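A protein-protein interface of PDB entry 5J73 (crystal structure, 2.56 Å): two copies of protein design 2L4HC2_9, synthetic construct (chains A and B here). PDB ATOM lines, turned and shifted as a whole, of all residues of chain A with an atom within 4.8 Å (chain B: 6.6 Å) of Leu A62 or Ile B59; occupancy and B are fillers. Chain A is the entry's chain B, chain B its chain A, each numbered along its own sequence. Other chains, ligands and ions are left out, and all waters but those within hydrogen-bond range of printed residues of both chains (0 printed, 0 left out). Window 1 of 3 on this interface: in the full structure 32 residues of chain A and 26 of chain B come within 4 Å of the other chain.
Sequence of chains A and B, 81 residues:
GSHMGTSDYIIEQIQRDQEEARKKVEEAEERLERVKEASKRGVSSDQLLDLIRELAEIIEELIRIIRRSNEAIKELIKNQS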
ATOM      1  N   VAL A  25     -17.310  24.695  25.897  1.00  0.00           N
ATOM      2  CA  VAL A  25     -17.412  23.443  26.642  1.00  0.00           C
ATOM      3  C   VAL A  25     -18.868  23.000  26.757  1.00  0.00           C
ATOM      4  O   VAL A  25     -19.170  21.814  26.615  1.00  0.00           O
ATOM      5  CB  VAL A  25     -16.777  23.564  28.049  1.00  0.00           C
ATOM      6  CG1 VAL A  25     -17.133  22.368  28.921  1.00  0.00           C
ATOM      7  CG2 VAL A  25     -15.269  23.682  27.935  1.00  0.00           C
ATOM      8  N   ALA A  28     -19.998  21.622  23.568  1.00  0.00           N
ATOM      9  CA  ALA A  28     -19.347  20.329  23.383  1.00  0.00           C
ATOM     10  C   ALA A  28     -20.029  19.235  24.205  1.00  0.00           C
ATOM     11  O   ALA A  28     -20.161  18.105  23.742  1.00  0.00           O
ATOM     12  CB  ALA A  28     -17.875  20.424  23.747  1.00  0.00           C
ATOM     13  N   LEU A  32     -21.722  16.109  22.645  1.00  0.00           N
ATOM     14  CA  LEU A  32     -21.358  14.778  23.108  1.00  0.00           C
ATOM     15  C   LEU A  32     -22.594  13.936  23.381  1.00  0.00           C
ATOM     16  O   LEU A  32     -22.675  12.777  22.981  1.00  0.00           O
ATOM     17  CB  LEU A  32     -20.506  14.867  24.376  1.00  0.00           C
ATOM     18  CG  LEU A  32     -19.992  13.547  24.962  1.00  0.00           C
ATOM     19  CD1 LEU A  32     -19.209  12.741  23.930  1.00  0.00           C
ATOM     20  CD2 LEU A  32     -19.145  13.800  26.198  1.00  0.00           C
ATOM     21  N   LEU A  55     -16.592  13.587  16.999  1.00  0.00           N
ATOM     22  CA  LEU A  55     -15.931  13.609  18.299  1.00  0.00           C
ATOM     23  C   LEU A  55     -14.464  13.993  18.137  1.00  0.00           C
ATOM     24  O   LEU A  55     -13.882  14.623  19.019  1.00  0.00           O
ATOM     25  CB  LEU A  55     -16.060  12.257  19.008  1.00  0.00           C
ATOM     26  CG  LEU A  55     -17.462  11.825  19.461  1.00  0.00           C
ATOM     27  CD1 LEU A  55     -17.360  10.644  20.415  1.00  0.00           C
ATOM     28  CD2 LEU A  55     -18.249  12.963  20.103  1.00  0.00           C
ATOM     29  N   ILE A  58     -14.385  17.685  18.127  1.00  0.00           N
ATOM     30  CA  ILE A  58     -14.569  18.263  19.450  1.00  0.00           C
ATOM     31  C   ILE A  58     -13.262  18.215  20.223  1.00  0.00           C
ATOM     32  O   ILE A  58     -12.847  19.205  20.826  1.00  0.00           O
ATOM     33  CB  ILE A  58     -15.668  17.518  20.235  1.00  0.00           C
ATOM     34  CG1 ILE A  58     -17.031  17.752  19.583  1.00  0.00           C
ATOM     35  CG2 ILE A  58     -15.676  17.937  21.711  1.00  0.00           C
ATOM     36  CD1 ILE A  58     -18.108  16.820  20.082  1.00  0.00           C
ATOM     37  N   ILE A  59     -12.613  17.057  20.182  1.00  0.00           N
ATOM     38  CA  ILE A  59     -11.383  16.835  20.928  1.00  0.00           C
ATOM     39  C   ILE A  59     -10.316  17.828  20.498  1.00  0.00           C
ATOM     40  O   ILE A  59      -9.669  18.455  21.333  1.00  0.00           O
ATOM     41  CB  ILE A  59     -10.873  15.391  20.732  1.00  0.00           C
ATOM     42  CG1 ILE A  59     -11.806  14.402  21.435  1.00  0.00           C
ATOM     43  CG2 ILE A  59      -9.446  15.234  21.250  1.00  0.00           C
ATOM     44  CD1 ILE A  59     -11.691  12.984  20.926  1.00  0.00           C
ATOM     45  N   GLU A  60     -10.153  17.985  19.191  1.00  0.00           N
ATOM     46  CA  GLU A  60      -9.142  18.886  18.659  1.00  0.00           C
ATOM     47  C   GLU A  60      -9.449  20.325  19.058  1.00  0.00           C
ATOM     48  O   GLU A  60      -8.539  21.114  19.306  1.00  0.00           O
ATOM     49  CB  GLU A  60      -9.054  18.753  17.139  1.00  0.00           C
ATOM     50  CG  GLU A  60      -7.876  17.897  16.677  1.00  0.00           C
ATOM     51  CD  GLU A  60      -8.123  17.185  15.355  1.00  0.00           C
ATOM     52  OE1 GLU A  60      -9.163  17.437  14.712  1.00  0.00           O
ATOM     53  OE2 GLU A  60      -7.266  16.367  14.958  1.00  0.00           O
ATOM     54  N   GLU A  61     -10.734  20.656  19.126  1.00  0.00           N
ATOM     55  CA  GLU A  61     -11.161  21.989  19.537  1.00  0.00           C
ATOM     56  C   GLU A  61     -10.882  22.238  21.022  1.00  0.00           C
ATOM     57  O   GLU A  61     -10.377  23.298  21.391  1.00  0.00           O
ATOM     58  CB  GLU A  61     -12.650  22.187  19.240  1.00  0.00           C
ATOM     59  CG  GLU A  61     -13.133  23.620  19.429  1.00  0.00           C
ATOM     60  CD  GLU A  61     -14.551  23.834  18.930  1.00  0.00           C
ATOM     61  OE1 GLU A  61     -15.206  22.843  18.543  1.00  0.00           O
ATOM     62  OE2 GLU A  61     -15.010  24.997  18.922  1.00  0.00           O
ATOM     63  N   LEU A  62     -11.216  21.271  21.872  1.00  0.00           N
ATOM     64  CA  LEU A  62     -10.968  21.404  23.304  1.00  0.00           C
ATOM     65  C   LEU A  62      -9.474  21.514  23.600  1.00  0.00           C
ATOM     66  O   LEU A  62      -9.075  22.185  24.552  1.00  0.00           O
ATOM     67  CB  LEU A  62     -11.566  20.229  24.084  1.00  0.00           C
ATOM     68  CG  LEU A  62     -13.093  20.092  24.115  1.00  0.00           C
ATOM     69  CD1 LEU A  62     -13.489  18.882  24.947  1.00  0.00           C
ATOM     70  CD2 LEU A  62     -13.767  21.344  24.656  1.00  0.00           C
ATOM     71  N   ILE A  63      -8.653  20.855  22.787  1.00  0.00           N
ATOM     72  CA  ILE A  63      -7.205  20.930  22.958  1.00  0.00           C
ATOM     73  C   ILE A  63      -6.715  22.342  22.652  1.00  0.00           C
ATOM     74  O   ILE A  63      -5.826  22.851  23.337  1.00  0.00           O
ATOM     75  CB  ILE A  63      -6.468  19.898  22.067  1.00  0.00           C
ATOM     76  CG1 ILE A  63      -6.716  18.483  22.602  1.00  0.00           C
ATOM     77  CG2 ILE A  63      -4.963  20.185  22.028  1.00  0.00           C
ATOM     78  CD1 ILE A  63      -6.096  17.375  21.775  1.00  0.00           C
ATOM     79  N   ARG A  64      -7.298  22.983  21.641  1.00  0.00           N
ATOM     80  CA  ARG A  64      -6.933  24.362  21.329  1.00  0.00           C
ATOM     81  C   ARG A  64      -7.250  25.262  22.519  1.00  0.00           C
ATOM     82  O   ARG A  64      -6.456  26.135  22.878  1.00  0.00           O
ATOM     83  CB  ARG A  64      -7.672  24.868  20.090  1.00  0.00           C
ATOM     84  CG  ARG A  64      -7.226  24.246  18.783  1.00  0.00           C
ATOM     85  CD  ARG A  64      -7.887  24.941  17.601  1.00  0.00           C
ATOM     86  NE  ARG A  64      -9.144  24.304  17.214  1.00  0.00           N
ATOM     87  CZ  ARG A  64      -9.237  23.222  16.446  1.00  0.00           C
ATOM     88  NH1 ARG A  64      -8.143  22.634  15.979  1.00  0.00           N
ATOM     89  NH2 ARG A  64     -10.431  22.724  16.150  1.00  0.00           N
ATOM     90  N   ILE A  65      -8.416  25.038  23.124  1.00  0.00           N
ATOM     91  CA  ILE A  65      -8.845  25.797  24.296  1.00  0.00           C
ATOM     92  C   ILE A  65      -7.873  25.573  25.445  1.00  0.00           C
ATOM     93  O   ILE A  65      -7.516  26.510  26.156  1.00  0.00           O
ATOM     94  CB  ILE A  65     -10.279  25.404  24.730  1.00  0.00           C
ATOM     95  CG1 ILE A  65     -11.300  25.964  23.742  1.00  0.00           C
ATOM     96  CG2 ILE A  65     -10.604  25.918  26.129  1.00  0.00           C
ATOM     97  CD1 ILE A  65     -12.625  25.230  23.752  1.00  0.00           C
ATOM     98  N   ILE A  66      -7.449  24.326  25.623  1.00  0.00           N
ATOM     99  CA  ILE A  66      -6.522  23.985  26.693  1.00  0.00           C
ATOM    100  C   ILE A  66      -5.175  24.657  26.470  1.00  0.00           C
ATOM    101  O   ILE A  66      -4.590  25.190  27.408  1.00  0.00           O
ATOM    102  CB  ILE A  66      -6.346  22.456  26.812  1.00  0.00           C
ATOM    103  CG1 ILE A  66      -7.621  21.830  27.379  1.00  0.00           C
ATOM    104  CG2 ILE A  66      -5.162  22.099  27.703  1.00  0.00           C
ATOM    105  CD1 ILE A  66      -7.818  20.385  26.996  1.00  0.00           C
ATOM    106  N   ILE B  52     -15.927   4.917  19.916  1.00  0.00           N
ATOM    107  CA  ILE B  52     -16.753   6.070  20.267  1.00  0.00           C
ATOM    108  C   ILE B  52     -16.816   6.254  21.785  1.00  0.00           C
ATOM    109  O   ILE B  52     -16.720   7.376  22.284  1.00  0.00           O
ATOM    110  CB  ILE B  52     -18.175   5.926  19.680  1.00  0.00           C
ATOM    111  CG1 ILE B  52     -18.113   6.072  18.156  1.00  0.00           C
ATOM    112  CG2 ILE B  52     -19.131   6.944  20.303  1.00  0.00           C
ATOM    113  CD1 ILE B  52     -19.448   5.936  17.443  1.00  0.00           C
ATOM    114  N   GLU B  54     -14.549   5.212  23.809  1.00  0.00           N
ATOM    115  CA  GLU B  54     -13.188   5.560  24.181  1.00  0.00           C
ATOM    116  C   GLU B  54     -12.942   7.062  23.982  1.00  0.00           C
ATOM    117  O   GLU B  54     -12.333   7.715  24.829  1.00  0.00           O
ATOM    118  CB  GLU B  54     -12.208   4.712  23.365  1.00  0.00           C
ATOM    119  CG  GLU B  54     -10.733   4.958  23.616  1.00  0.00           C
ATOM    120  CD  GLU B  54      -9.858   3.944  22.888  1.00  0.00           C
ATOM    121  OE1 GLU B  54     -10.413   3.050  22.212  1.00  0.00           O
ATOM    122  OE2 GLU B  54      -8.618   4.033  22.987  1.00  0.00           O
ATOM    123  N   LEU B  55     -13.417   7.606  22.865  1.00  0.00           N
ATOM    124  CA  LEU B  55     -13.291   9.039  22.592  1.00  0.00           C
ATOM    125  C   LEU B  55     -14.162   9.881  23.525  1.00  0.00           C
ATOM    126  O   LEU B  55     -13.784  10.993  23.904  1.00  0.00           O
ATOM    127  CB  LEU B  55     -13.656   9.349  21.137  1.00  0.00           C
ATOM    128  CG  LEU B  55     -12.732   8.825  20.029  1.00  0.00           C
ATOM    129  CD1 LEU B  55     -13.079   9.489  18.706  1.00  0.00           C
ATOM    130  CD2 LEU B  55     -11.258   9.034  20.355  1.00  0.00           C
ATOM    131  N   ALA B  56     -15.327   9.357  23.887  1.00  0.00           N
ATOM    132  CA  ALA B  56     -16.219  10.050  24.810  1.00  0.00           C
ATOM    133  C   ALA B  56     -15.549  10.216  26.170  1.00  0.00           C
ATOM    134  O   ALA B  56     -15.755  11.215  26.855  1.00  0.00           O
ATOM    135  CB  ALA B  56     -17.532   9.298  24.951  1.00  0.00           C
ATOM    136  N   GLU B  57     -14.749   9.228  26.557  1.00  0.00           N
ATOM    137  CA  GLU B  57     -13.990   9.300  27.797  1.00  0.00           C
ATOM    138  C   GLU B  57     -12.981  10.432  27.727  1.00  0.00           C
ATOM    139  O   GLU B  57     -12.793  11.176  28.690  1.00  0.00           O
ATOM    140  CB  GLU B  57     -13.259   7.987  28.065  1.00  0.00           C
ATOM    141  CG  GLU B  57     -14.077   6.944  28.788  1.00  0.00           C
ATOM    142  CD  GLU B  57     -13.253   5.721  29.135  1.00  0.00           C
ATOM    143  OE1 GLU B  57     -12.136   5.583  28.592  1.00  0.00           O
ATOM    144  OE2 GLU B  57     -13.723   4.892  29.943  1.00  0.00           O
ATOM    145  N   ILE B  58     -12.324  10.542  26.578  1.00  0.00           N
ATOM    146  CA  ILE B  58     -11.315  11.566  26.361  1.00  0.00           C
ATOM    147  C   ILE B  58     -11.933  12.951  26.462  1.00  0.00           C
ATOM    148  O   ILE B  58     -11.383  13.829  27.120  1.00  0.00           O
ATOM    149  CB  ILE B  58     -10.629  11.383  24.992  1.00  0.00           C
ATOM    150  CG1 ILE B  58      -9.727  10.152  25.035  1.00  0.00           C
ATOM    151  CG2 ILE B  58      -9.810  12.615  24.612  1.00  0.00           C
ATOM    152  CD1 ILE B  58      -9.243   9.692  23.683  1.00  0.00           C
ATOM    153  N   ILE B  59     -13.078  13.140  25.818  1.00  0.00           N
ATOM    154  CA  ILE B  59     -13.729  14.441  25.806  1.00  0.00           C
ATOM    155  C   ILE B  59     -14.046  14.871  27.231  1.00  0.00           C
ATOM    156  O   ILE B  59     -13.771  16.003  27.624  1.00  0.00           O
ATOM    157  CB  ILE B  59     -15.013  14.419  24.957  1.00  0.00           C
ATOM    158  CG1 ILE B  59     -14.653  14.294  23.477  1.00  0.00           C
ATOM    159  CG2 ILE B  59     -15.857  15.672  25.201  1.00  0.00           C
ATOM    160  CD1 ILE B  59     -15.788  13.803  22.608  1.00  0.00           C
ATOM    161  N   GLU B  60     -14.602  13.952  28.010  1.00  0.00           N
ATOM    162  CA  GLU B  60     -14.974  14.249  29.386  1.00  0.00           C
ATOM    163  C   GLU B  60     -13.750  14.581  30.239  1.00  0.00           C
ATOM    164  O   GLU B  60     -13.814  15.439  31.118  1.00  0.00           O
ATOM    165  CB  GLU B  60     -15.743  13.070  29.980  1.00  0.00           C
ATOM    166  CG  GLU B  60     -17.246  13.302  30.012  1.00  0.00           C
ATOM    167  CD  GLU B  60     -18.055  12.027  29.879  1.00  0.00           C
ATOM    168  OE1 GLU B  60     -17.464  10.928  29.868  1.00  0.00           O
ATOM    169  OE2 GLU B  60     -19.294  12.127  29.786  1.00  0.00           O
ATOM    170  N   GLU B  61     -12.634  13.915  29.965  1.00  0.00           N
ATOM    171  CA  GLU B  61     -11.392  14.188  30.678  1.00  0.00           C
ATOM    172  C   GLU B  61     -10.875  15.571  30.302  1.00  0.00           C
ATOM    173  O   GLU B  61     -10.446  16.340  31.163  1.00  0.00           O
ATOM    174  CB  GLU B  61     -10.341  13.118  30.371  1.00  0.00           C
ATOM    175  CG  GLU B  61     -10.561  11.813  31.125  1.00  0.00           C
ATOM    176  CD  GLU B  61      -9.553  10.741  30.755  1.00  0.00           C
ATOM    177  OE1 GLU B  61      -8.916  10.858  29.686  1.00  0.00           O
ATOM    178  OE2 GLU B  61      -9.398   9.778  31.538  1.00  0.00           O
ATOM    179  N   LEU B  62     -10.905  15.871  29.009  1.00  0.00           N
ATOM    180  CA  LEU B  62     -10.478  17.173  28.513  1.00  0.00           C
ATOM    181  C   LEU B  62     -11.365  18.295  29.057  1.00  0.00           C
ATOM    182  O   LEU B  62     -10.897  19.409  29.279  1.00  0.00           O
ATOM    183  CB  LEU B  62     -10.491  17.185  26.984  1.00  0.00           C
ATOM    184  CG  LEU B  62      -9.486  16.267  26.279  1.00  0.00           C
ATOM    185  CD1 LEU B  62      -9.635  16.383  24.775  1.00  0.00           C
ATOM    186  CD2 LEU B  62      -8.052  16.573  26.695  1.00  0.00           C
ATOM    187  N   ILE B  63     -12.644  18.000  29.265  1.00  0.00           N
ATOM    188  CA  ILE B  63     -13.568  18.984  29.821  1.00  0.00           C
ATOM    189  C   ILE B  63     -13.241  19.308  31.277  1.00  0.00           C
ATOM    190  O   ILE B  63     -13.343  20.461  31.688  1.00  0.00           O
ATOM    191  CB  ILE B  63     -15.033  18.506  29.696  1.00  0.00           C
ATOM    192  CG1 ILE B  63     -15.467  18.589  28.228  1.00  0.00           C
ATOM    193  CG2 ILE B  63     -15.965  19.365  30.555  1.00  0.00           C
ATOM    194  CD1 ILE B  63     -16.863  18.080  27.947  1.00  0.00           C
ATOM    195  N   ARG B  64     -12.850  18.302  32.056  1.00  0.00           N
ATOM    196  CA  ARG B  64     -12.441  18.540  33.439  1.00  0.00           C
ATOM    197  C   ARG B  64     -11.227  19.456  33.492  1.00  0.00           C
ATOM    198  O   ARG B  64     -11.144  20.340  34.340  1.00  0.00           O
ATOM    199  CB  ARG B  64     -12.122  17.230  34.157  1.00  0.00           C
ATOM    200  CG  ARG B  64     -13.333  16.386  34.485  1.00  0.00           C
ATOM    201  CD  ARG B  64     -12.945  15.182  35.323  1.00  0.00           C
ATOM    202  NE  ARG B  64     -12.664  14.030  34.473  1.00  0.00           N
ATOM    203  CZ  ARG B  64     -13.596  13.233  33.964  1.00  0.00           C
ATOM    204  NH1 ARG B  64     -14.880  13.456  34.214  1.00  0.00           N
ATOM    205  NH2 ARG B  64     -13.243  12.217  33.191  1.00  0.00           N
ATOM    206  N   ILE B  66     -10.326  21.745  31.356  1.00  0.00           N
ATOM    207  CA  ILE B  66     -10.704  23.116  31.036  1.00  0.00           C
ATOM    208  C   ILE B  66     -11.339  23.778  32.251  1.00  0.00           C
ATOM    209  O   ILE B  66     -11.082  24.947  32.529  1.00  0.00           O
ATOM    210  CB  ILE B  66     -11.658  23.174  29.830  1.00  0.00           C
ATOM    211  CG1 ILE B  66     -10.899  22.822  28.552  1.00  0.00           C
ATOM    212  CG2 ILE B  66     -12.283  24.555  29.684  1.00  0.00           C
ATOM    213  CD1 ILE B  66     -11.773  22.267  27.459  1.00  0.00           C
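Printed residues of chain A that touch a printed residue of chain B: Val A25, Leu A32, Leu A55, Ile A59, Leu A62, Ile A65 and Ile A66. Hydrophobic or aromatic side chains of chain B within 4 Å of the printed part of chain A: Leu B55, Ala B56, Ile B59, Leu B62, Ile B63 and Ile B66. Among the printed residues, 16 pairs touch across the chains.
Leu A55 touches its own counterpart, Leu B55. Leu A55 touches Ile B59, but with the chains exchanged Ile A59 does not touch Leu B55 (4.01 Å). Ile A59 touches its own counterpart, Ile B59. Leu A62 touches Ile B66, and with the chains exchanged Ile A66 touches Leu B62. Of the 16 pairs that touch across the chains among the printed residues, 7 have their exchanged pair printed and touching as well.
Ile B63 touches Val A25 (CG2 to CG1, 3.6 Å). Leu A32 touches Ile B59 (CD1 to CD1, 3.8 Å). OE2 of Glu B60 touches CD2 of Leu A32 (3.96 Å). CD1 of Ile B59 touches CD2 of Leu A55 (3.6 Å). CG1 of Ile B59 touches CG1 of Ile A59, at 3.5 Å. Ile A59 touches Leu B62. CD1 of Leu A62 touches CG1 of Ile B63, at 3.8 Å. CG1 of Ile B66 touches CG2 of Ile A65 (3.9 Å). Leu B62 touches Ile A66 (CD2 to CD1, 3.8 Å). CG1 of Ile A66 touches CG1 of Ile B66, at 3.6 Å.
Of the printed residues of chain B, Leu A62 touches Ile B59 (3.9 Å), Ile B63 (3.8 Å) and Ile B66 (3.6 Å). Printed residues of chain A within 4 Å of Leu B62: Ile A59 and Ile A66. Of the printed residues of chain B, Ile A65 touches Ile B66 (3.9 Å). Of the printed residues of chain A, Ile B63 touches Val A25 and Leu A62. Printed residues of chain B within 4 Å of Leu A55: Ile B52, Leu B55 and Ile B59. The nearest printed residue of chain B that does not touch Val A25 is Leu B62 (6.3 Å).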
